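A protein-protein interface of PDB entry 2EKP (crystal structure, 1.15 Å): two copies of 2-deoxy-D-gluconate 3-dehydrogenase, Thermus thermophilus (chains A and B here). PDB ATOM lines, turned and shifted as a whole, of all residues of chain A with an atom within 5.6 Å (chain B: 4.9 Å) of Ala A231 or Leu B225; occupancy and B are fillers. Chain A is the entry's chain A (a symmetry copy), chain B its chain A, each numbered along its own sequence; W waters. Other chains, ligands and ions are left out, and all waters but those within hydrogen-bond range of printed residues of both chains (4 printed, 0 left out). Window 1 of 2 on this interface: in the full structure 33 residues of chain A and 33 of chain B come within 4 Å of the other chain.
Position printed for both chains: 230.
Of the 11 pairs that touch across the chains among the printed residues, none has its exchanged pair printed and touching as well.
The guanidinium group (NH2) of Arg B168 is in salt-bridge range of the side-chain carboxylate (OE2) of Glu B223.
O of Leu B225 sits at hydrogen-bond distance from ND2 of Asn B170.
N of Gln B228 is in hydrogen-bond range of OD1 of Asn B170, 3.1 Å away.
The backbone NH (N) of Val A232 lies within hydrogen-bond range of the backbone carbonyl oxygen (O) of Cys A173 (2.9 Å).
The backbone NH of Met A201 lies within hydrogen-bond range of the backbone carbonyl oxygen of Gly A234.
The backbone NH (N) of Leu A237 sits at hydrogen-bond distance from the side-chain carboxylate (OD2) of Asp A233, 2.8 Å away.
Of chain B, only Leu B225 (3.5 Å) and Gln B228 (3.5 Å) come within 4 Å of Ala A231.
Leu B225 touches just one residue of chain A: Ala A231.
Of the printed residues of chain B, Asp A233 touches Tyr B224 and Thr B226.
Of the printed residues of chain A, Arg B168 touches Met A201 (3.2 Å).
Of the printed residues of chain A, Tyr B224 touches Met A201, Val A232, Asp A233 and Gly A234.
Val B230 touches none of the printed residues of chain A.
The nearest residue of chain A that does not touch Leu B225 is Val A232 (4.1 Å).
The nearest printed residue of chain A that does not touch Tyr B224 is Ala A231 (5.3 Å).
Water W3 bridges OE1 of Gln B228 (2.8 Å) and N of Ala A231 (3.0 Å).
Water W1 lies within hydrogen-bond range of the side-chain carboxylate of Asp A233 (2.8 Å), the backbone carbonyl oxygen of Ala A231 (2.8 Å) and the backbone NH of Thr B226 (3.0 Å).
Water W4 lies within hydrogen-bond range of the side-chain carboxylate of Asp A233 (2.8 Å), the side-chain amide nitrogen of Gln B228 (2.9 Å) and the backbone carbonyl oxygen of Thr B226 (2.9 Å).
Water W2 lies within hydrogen-bond range of O of Asp A233 (2.8 Å) and OH of Tyr B224 (2.9 Å).
Met A201 touches Tyr B224 (CE to CD1, 3.7 Å).
O of Ala A231 touches CG of Leu B225 (3.5 Å).
CG of Gln B228 touches O of Ala A231 (3.5 Å).
Val A232 touches Tyr B224.
Thr B226 touches Asp A233 (O to OD1, 3.9 Å).
C of Gly A234 touches CG2 of Thr B226 (3.6 Å).
Gln B228 touches Leu A237 (NE2 to CB, 3.8 Å).
The guanidinium group (NE) of Arg B168 lies close to the side-chain sulfur (SD) of Met A201 (3.6 Å).
The backbone carbonyl oxygen (O) of Tyr B224 is in hydrogen-bond range of the backbone NH (N) of Asp A233 (3.3 Å).
The backbone NH (N) of Gly A234 sits at hydrogen-bond distance from the backbone carbonyl oxygen (O) of Tyr B224, at 2.9 Å.
SD of Met A201 sits close to O of Glu B223 (3.4 Å).
Hydrophobic or aromatic side chains of chain B within 4 Å of the printed part of chain A: Tyr B224 and Leu B225.
Printed residues of chain A that touch a printed residue of chain B: Met A201, Ala A231, Val A232, Asp A233, Gly A234 and Leu A237.
Among the printed residues, 11 pairs touch across the chains.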
ATOM      1  N   PHE A 133      -4.244   2.126   7.559  1.00  0.00           N
ATOM      2  CA  PHE A 133      -3.996   3.558   7.402  1.00  0.00           C
ATOM      3  C   PHE A 133      -4.740   4.469   8.377  1.00  0.00           C
ATOM      4  O   PHE A 133      -4.450   5.665   8.448  1.00  0.00           O
ATOM      5  CB  PHE A 133      -4.354   3.961   5.972  1.00  0.00           C
ATOM      6  CG  PHE A 133      -3.599   3.193   4.929  1.00  0.00           C
ATOM      7  CD1 PHE A 133      -2.270   3.495   4.661  1.00  0.00           C
ATOM      8  CD2 PHE A 133      -4.195   2.137   4.247  1.00  0.00           C
ATOM      9  CE1 PHE A 133      -1.542   2.763   3.728  1.00  0.00           C
ATOM     10  CE2 PHE A 133      -3.475   1.395   3.309  1.00  0.00           C
ATOM     11  CZ  PHE A 133      -2.145   1.710   3.053  1.00  0.00           C
ATOM     12  N   LEU A 171      -0.088  -6.263  -0.225  1.00  0.00           N
ATOM     13  CA  LEU A 171      -1.119  -6.190   0.795  1.00  0.00           C
ATOM     14  C   LEU A 171      -2.408  -5.626   0.212  1.00  0.00           C
ATOM     15  O   LEU A 171      -2.490  -4.437  -0.095  1.00  0.00           O
ATOM     16  CB  LEU A 171      -0.639  -5.296   1.944  1.00  0.00           C
ATOM     17  CG  LEU A 171      -1.545  -5.176   3.173  1.00  0.00           C
ATOM     18  CD1 LEU A 171      -1.563  -6.493   3.937  1.00  0.00           C
ATOM     19  CD2 LEU A 171      -1.030  -4.059   4.072  1.00  0.00           C
ATOM     20  N   CYS A 173      -5.834  -4.187   0.635  1.00  0.00           N
ATOM     21  CA  CYS A 173      -6.538  -3.527   1.727  1.00  0.00           C
ATOM     22  C   CYS A 173      -7.979  -3.217   1.369  1.00  0.00           C
ATOM     23  O   CYS A 173      -8.276  -2.173   0.788  1.00  0.00           O
ATOM     24  CB  CYS A 173      -5.811  -2.237   2.108  1.00  0.00           C
ATOM     25  SG  CYS A 173      -4.147  -2.507   2.733  1.00  0.00           S
ATOM     26  N   PRO A 174      -8.898  -4.129   1.706  1.00  0.00           N
ATOM     27  CA  PRO A 174     -10.308  -3.898   1.395  1.00  0.00           C
ATOM     28  C   PRO A 174     -10.898  -2.830   2.301  1.00  0.00           C
ATOM     29  O   PRO A 174     -10.409  -2.601   3.414  1.00  0.00           O
ATOM     30  CB  PRO A 174     -10.964  -5.253   1.665  1.00  0.00           C
ATOM     31  CG  PRO A 174      -9.823  -6.235   1.611  1.00  0.00           C
ATOM     32  CD  PRO A 174      -8.698  -5.479   2.256  1.00  0.00           C
ATOM     33  N   MET A 201     -18.631   5.965  -2.971  1.00  0.00           N
ATOM     34  CA  MET A 201     -19.525   5.135  -3.766  1.00  0.00           C
ATOM     35  C   MET A 201     -20.873   4.907  -3.084  1.00  0.00           C
ATOM     36  O   MET A 201     -21.815   4.419  -3.708  1.00  0.00           O
ATOM     37  CB  MET A 201     -18.851   3.807  -4.116  1.00  0.00           C
ATOM     38  CG  MET A 201     -17.852   3.963  -5.254  1.00  0.00           C
ATOM     39  SD  MET A 201     -17.048   2.442  -5.775  1.00  0.00           S
ATOM     40  CE  MET A 201     -18.464   1.433  -6.192  1.00  0.00           C
ATOM     41  N   VAL A 213      -9.595  -7.766  -7.671  1.00  0.00           N
ATOM     42  CA  VAL A 213      -8.278  -7.163  -7.522  1.00  0.00           C
ATOM     43  C   VAL A 213      -7.293  -8.171  -6.935  1.00  0.00           C
ATOM     44  O   VAL A 213      -6.125  -8.200  -7.317  1.00  0.00           O
ATOM     45  CB  VAL A 213      -8.351  -5.899  -6.630  1.00  0.00           C
ATOM     46  CG1 VAL A 213      -6.979  -5.246  -6.529  1.00  0.00           C
ATOM     47  CG2 VAL A 213      -9.366  -4.919  -7.209  1.00  0.00           C
ATOM     48  N   ALA A 229       0.730  -1.752  -0.879  1.00  0.00           N
ATOM     49  CA  ALA A 229      -0.618  -1.915  -0.373  1.00  0.00           C
ATOM     50  C   ALA A 229      -1.493  -1.397  -1.518  1.00  0.00           C
ATOM     51  O   ALA A 229      -1.149  -0.408  -2.179  1.00  0.00           O
ATOM     52  CB  ALA A 229      -0.833  -1.068   0.873  1.00  0.00           C
ATOM     53  N   VAL A 230      -2.593  -2.091  -1.777  1.00  0.00           N
ATOM     54  CA  VAL A 230      -3.535  -1.686  -2.811  1.00  0.00           C
ATOM     55  C   VAL A 230      -4.883  -1.636  -2.107  1.00  0.00           C
ATOM     56  O   VAL A 230      -5.414  -2.669  -1.698  1.00  0.00           O
ATOM     57  CB  VAL A 230      -3.590  -2.704  -3.972  1.00  0.00           C
ATOM     58  CG1 VAL A 230      -4.620  -2.259  -5.001  1.00  0.00           C
ATOM     59  CG2 VAL A 230      -2.213  -2.831  -4.617  1.00  0.00           C
ATOM     60  N   ALA A 231      -5.414  -0.428  -1.941  1.00  0.00           N
ATOM     61  CA  ALA A 231      -6.688  -0.236  -1.258  1.00  0.00           C
ATOM     62  C   ALA A 231      -7.866  -0.271  -2.223  1.00  0.00           C
ATOM     63  O   ALA A 231      -7.895   0.457  -3.214  1.00  0.00           O
ATOM     64  CB  ALA A 231      -6.676   1.085  -0.493  1.00  0.00           C
ATOM     65  N   VAL A 232      -8.832  -1.129  -1.914  1.00  0.00           N
ATOM     66  CA  VAL A 232     -10.042  -1.308  -2.718  1.00  0.00           C
ATOM     67  C   VAL A 232     -11.155  -0.999  -1.722  1.00  0.00           C
ATOM     68  O   VAL A 232     -11.716  -1.897  -1.083  1.00  0.00           O
ATOM     69  CB  VAL A 232     -10.122  -2.763  -3.225  1.00  0.00           C
ATOM     70  CG1 VAL A 232     -11.306  -2.936  -4.150  1.00  0.00           C
ATOM     71  CG2 VAL A 232      -8.825  -3.126  -3.942  1.00  0.00           C
ATOM     72  N   ASP A 233     -11.475   0.287  -1.613  1.00  0.00           N
ATOM     73  CA  ASP A 233     -12.413   0.760  -0.606  1.00  0.00           C
ATOM     74  C   ASP A 233     -13.535   1.698  -1.025  1.00  0.00           C
ATOM     75  O   ASP A 233     -14.094   2.393  -0.175  1.00  0.00           O
ATOM     76  CB  ASP A 233     -11.611   1.444   0.503  1.00  0.00           C
ATOM     77  CG  ASP A 233     -10.954   2.741   0.034  1.00  0.00           C
ATOM     78  OD1 ASP A 233     -11.104   3.105  -1.158  1.00  0.00           O
ATOM     79  OD2 ASP A 233     -10.289   3.401   0.861  1.00  0.00           O
ATOM     80  N   GLY A 234     -13.858   1.736  -2.312  1.00  0.00           N
ATOM     81  CA  GLY A 234     -14.934   2.598  -2.769  1.00  0.00           C
ATOM     82  C   GLY A 234     -14.705   4.083  -2.562  1.00  0.00           C
ATOM     83  O   GLY A 234     -15.641   4.882  -2.654  1.00  0.00           O
ATOM     84  N   LEU A 237     -10.821   5.935   1.960  1.00  0.00           N
ATOM     85  CA  LEU A 237      -9.615   6.609   2.421  1.00  0.00           C
ATOM     86  C   LEU A 237      -9.387   7.956   1.752  1.00  0.00           C
ATOM     87  O   LEU A 237      -8.850   8.876   2.367  1.00  0.00           O
ATOM     88  CB  LEU A 237      -8.399   5.703   2.217  1.00  0.00           C
ATOM     89  CG  LEU A 237      -8.389   4.447   3.098  1.00  0.00           C
ATOM     90  CD1 LEU A 237      -7.261   3.527   2.656  1.00  0.00           C
ATOM     91  CD2 LEU A 237      -8.235   4.835   4.568  1.00  0.00           C
ATOM     92  N   ARG B 168     -14.468   5.954 -11.787  1.00  0.00           N
ATOM     93  CA  ARG B 168     -13.398   5.616 -10.858  1.00  0.00           C
ATOM     94  C   ARG B 168     -12.191   6.430 -11.329  1.00  0.00           C
ATOM     95  O   ARG B 168     -11.947   6.548 -12.535  1.00  0.00           O
ATOM     96  CB  ARG B 168     -13.091   4.118 -10.901  1.00  0.00           C
ATOM     97  CG  ARG B 168     -14.319   3.230 -10.723  1.00  0.00           C
ATOM     98  CD  ARG B 168     -14.975   3.401  -9.357  1.00  0.00           C
ATOM     99  NE  ARG B 168     -16.272   2.728  -9.301  1.00  0.00           N
ATOM    100  CZ  ARG B 168     -17.445   3.354  -9.251  1.00  0.00           C
ATOM    101  NH1 ARG B 168     -17.501   4.680  -9.248  1.00  0.00           N
ATOM    102  NH2 ARG B 168     -18.568   2.651  -9.197  1.00  0.00           N
ATOM    103  N   ASN B 170      -8.034   6.942 -10.536  1.00  0.00           N
ATOM    104  CA  ASN B 170      -6.858   6.444  -9.834  1.00  0.00           C
ATOM    105  C   ASN B 170      -5.573   6.971 -10.446  1.00  0.00           C
ATOM    106  O   ASN B 170      -5.568   7.515 -11.554  1.00  0.00           O
ATOM    107  CB  ASN B 170      -6.859   4.914  -9.829  1.00  0.00           C
ATOM    108  CG  ASN B 170      -8.018   4.341  -9.039  1.00  0.00           C
ATOM    109  OD1 ASN B 170      -8.064   4.461  -7.815  1.00  0.00           O
ATOM    110  ND2 ASN B 170      -8.970   3.730  -9.738  1.00  0.00           N
ATOM    111  N   LEU B 217      -6.924  -1.031 -14.064  1.00  0.00           N
ATOM    112  CA  LEU B 217      -7.503   0.200 -13.537  1.00  0.00           C
ATOM    113  C   LEU B 217      -8.457   0.874 -14.525  1.00  0.00           C
ATOM    114  O   LEU B 217      -9.146   1.836 -14.177  1.00  0.00           O
ATOM    115  CB  LEU B 217      -6.383   1.161 -13.119  1.00  0.00           C
ATOM    116  CG  LEU B 217      -5.515   0.647 -11.964  1.00  0.00           C
ATOM    117  CD1 LEU B 217      -4.367   1.606 -11.710  1.00  0.00           C
ATOM    118  CD2 LEU B 217      -6.363   0.486 -10.711  1.00  0.00           C
ATOM    119  N   ALA B 222     -11.663  -2.639 -11.374  1.00  0.00           N
ATOM    120  CA  ALA B 222     -11.598  -1.479 -10.492  1.00  0.00           C
ATOM    121  C   ALA B 222     -12.961  -0.951 -10.057  1.00  0.00           C
ATOM    122  O   ALA B 222     -13.073   0.195  -9.619  1.00  0.00           O
ATOM    123  CB  ALA B 222     -10.802  -0.362 -11.168  1.00  0.00           C
ATOM    124  N   GLU B 223     -13.992  -1.781 -10.153  1.00  0.00           N
ATOM    125  CA  GLU B 223     -15.332  -1.352  -9.767  1.00  0.00           C
ATOM    126  C   GLU B 223     -15.394  -0.733  -8.370  1.00  0.00           C
ATOM    127  O   GLU B 223     -16.109   0.246  -8.160  1.00  0.00           O
ATOM    128  CB  GLU B 223     -16.308  -2.529  -9.866  1.00  0.00           C
ATOM    129  CG  GLU B 223     -17.735  -2.243  -9.396  1.00  0.00           C
ATOM    130  CD  GLU B 223     -18.316  -0.959  -9.962  1.00  0.00           C
ATOM    131  OE1 GLU B 223     -18.059  -0.645 -11.139  1.00  0.00           O
ATOM    132  OE2 GLU B 223     -19.047  -0.261  -9.230  1.00  0.00           O
ATOM    133  N   TYR B 224     -14.643  -1.283  -7.418  1.00  0.00           N
ATOM    134  CA  TYR B 224     -14.659  -0.745  -6.059  1.00  0.00           C
ATOM    135  C   TYR B 224     -13.310  -0.124  -5.687  1.00  0.00           C
ATOM    136  O   TYR B 224     -13.014   0.070  -4.506  1.00  0.00           O
ATOM    137  CB  TYR B 224     -15.017  -1.851  -5.052  1.00  0.00           C
ATOM    138  CG  TYR B 224     -15.654  -1.345  -3.772  1.00  0.00           C
ATOM    139  CD1 TYR B 224     -16.964  -0.872  -3.767  1.00  0.00           C
ATOM    140  CD2 TYR B 224     -14.945  -1.328  -2.569  1.00  0.00           C
ATOM    141  CE1 TYR B 224     -17.556  -0.391  -2.601  1.00  0.00           C
ATOM    142  CE2 TYR B 224     -15.528  -0.847  -1.394  1.00  0.00           C
ATOM    143  CZ  TYR B 224     -16.833  -0.381  -1.417  1.00  0.00           C
ATOM    144  OH  TYR B 224     -17.402   0.096  -0.256  1.00  0.00           O
ATOM    145  N   LEU B 225     -12.504   0.199  -6.696  1.00  0.00           N
ATOM    146  CA  LEU B 225     -11.183   0.775  -6.474  1.00  0.00           C
ATOM    147  C   LEU B 225     -11.141   2.194  -7.032  1.00  0.00           C
ATOM    148  O   LEU B 225     -11.164   2.394  -8.251  1.00  0.00           O
ATOM    149  CB  LEU B 225     -10.121  -0.096  -7.156  1.00  0.00           C
ATOM    150  CG  LEU B 225      -8.681  -0.024  -6.640  1.00  0.00           C
ATOM    151  CD1 LEU B 225      -7.845  -1.086  -7.341  1.00  0.00           C
ATOM    152  CD2 LEU B 225      -8.100   1.363  -6.866  1.00  0.00           C
ATOM    153  N   THR B 226     -11.091   3.181  -6.145  1.00  0.00           N
ATOM    154  CA  THR B 226     -11.055   4.559  -6.597  1.00  0.00           C
ATOM    155  C   THR B 226     -10.405   5.502  -5.584  1.00  0.00           C
ATOM    156  O   THR B 226     -10.442   5.254  -4.374  1.00  0.00           O
ATOM    157  CB  THR B 226     -12.480   5.042  -6.953  1.00  0.00           C
ATOM    158  OG1 THR B 226     -12.388   6.267  -7.685  1.00  0.00           O
ATOM    159  CG2 THR B 226     -13.329   5.244  -5.699  1.00  0.00           C
ATOM    160  N   GLY B 227      -9.794   6.568  -6.101  1.00  0.00           N
ATOM    161  CA  GLY B 227      -9.128   7.565  -5.275  1.00  0.00           C
ATOM    162  C   GLY B 227      -7.793   7.106  -4.730  1.00  0.00           C
ATOM    163  O   GLY B 227      -7.302   7.651  -3.740  1.00  0.00           O
ATOM    164  N   GLN B 228      -7.187   6.135  -5.404  1.00  0.00           N
ATOM    165  CA  GLN B 228      -5.933   5.555  -4.953  1.00  0.00           C
ATOM    166  C   GLN B 228      -4.767   5.610  -5.916  1.00  0.00           C
ATOM    167  O   GLN B 228      -4.935   5.693  -7.135  1.00  0.00           O
ATOM    168  CB  GLN B 228      -6.157   4.083  -4.603  1.00  0.00           C
ATOM    169  CG  GLN B 228      -6.987   3.849  -3.372  1.00  0.00           C
ATOM    170  CD  GLN B 228      -6.285   4.335  -2.130  1.00  0.00           C
ATOM    171  OE1 GLN B 228      -5.106   4.048  -1.925  1.00  0.00           O
ATOM    172  NE2 GLN B 228      -6.998   5.072  -1.291  1.00  0.00           N
ATOM    173  N   VAL B 230      -1.528   3.475  -7.185  1.00  0.00           N
ATOM    174  CA  VAL B 230      -1.104   2.084  -7.268  1.00  0.00           C
ATOM    175  C   VAL B 230       0.300   2.143  -7.849  1.00  0.00           C
ATOM    176  O   VAL B 230       0.483   2.513  -9.009  1.00  0.00           O
ATOM    177  CB  VAL B 230      -2.020   1.257  -8.197  1.00  0.00           C
ATOM    178  CG1 VAL B 230      -1.509  -0.174  -8.286  1.00  0.00           C
ATOM    179  CG2 VAL B 230      -3.451   1.280  -7.670  1.00  0.00           C
HETATM  180  O   HOH W   1     -10.160   2.055  -3.535  1.00  0.00           O
HETATM  181  O   HOH W   2     -15.445   0.798   1.741  1.00  0.00           O
HETATM  182  O   HOH W   3      -3.832   1.849  -3.009  1.00  0.00           O
HETATM  183  O   HOH W   4      -9.808   5.582  -1.579  1.00  0.00           O
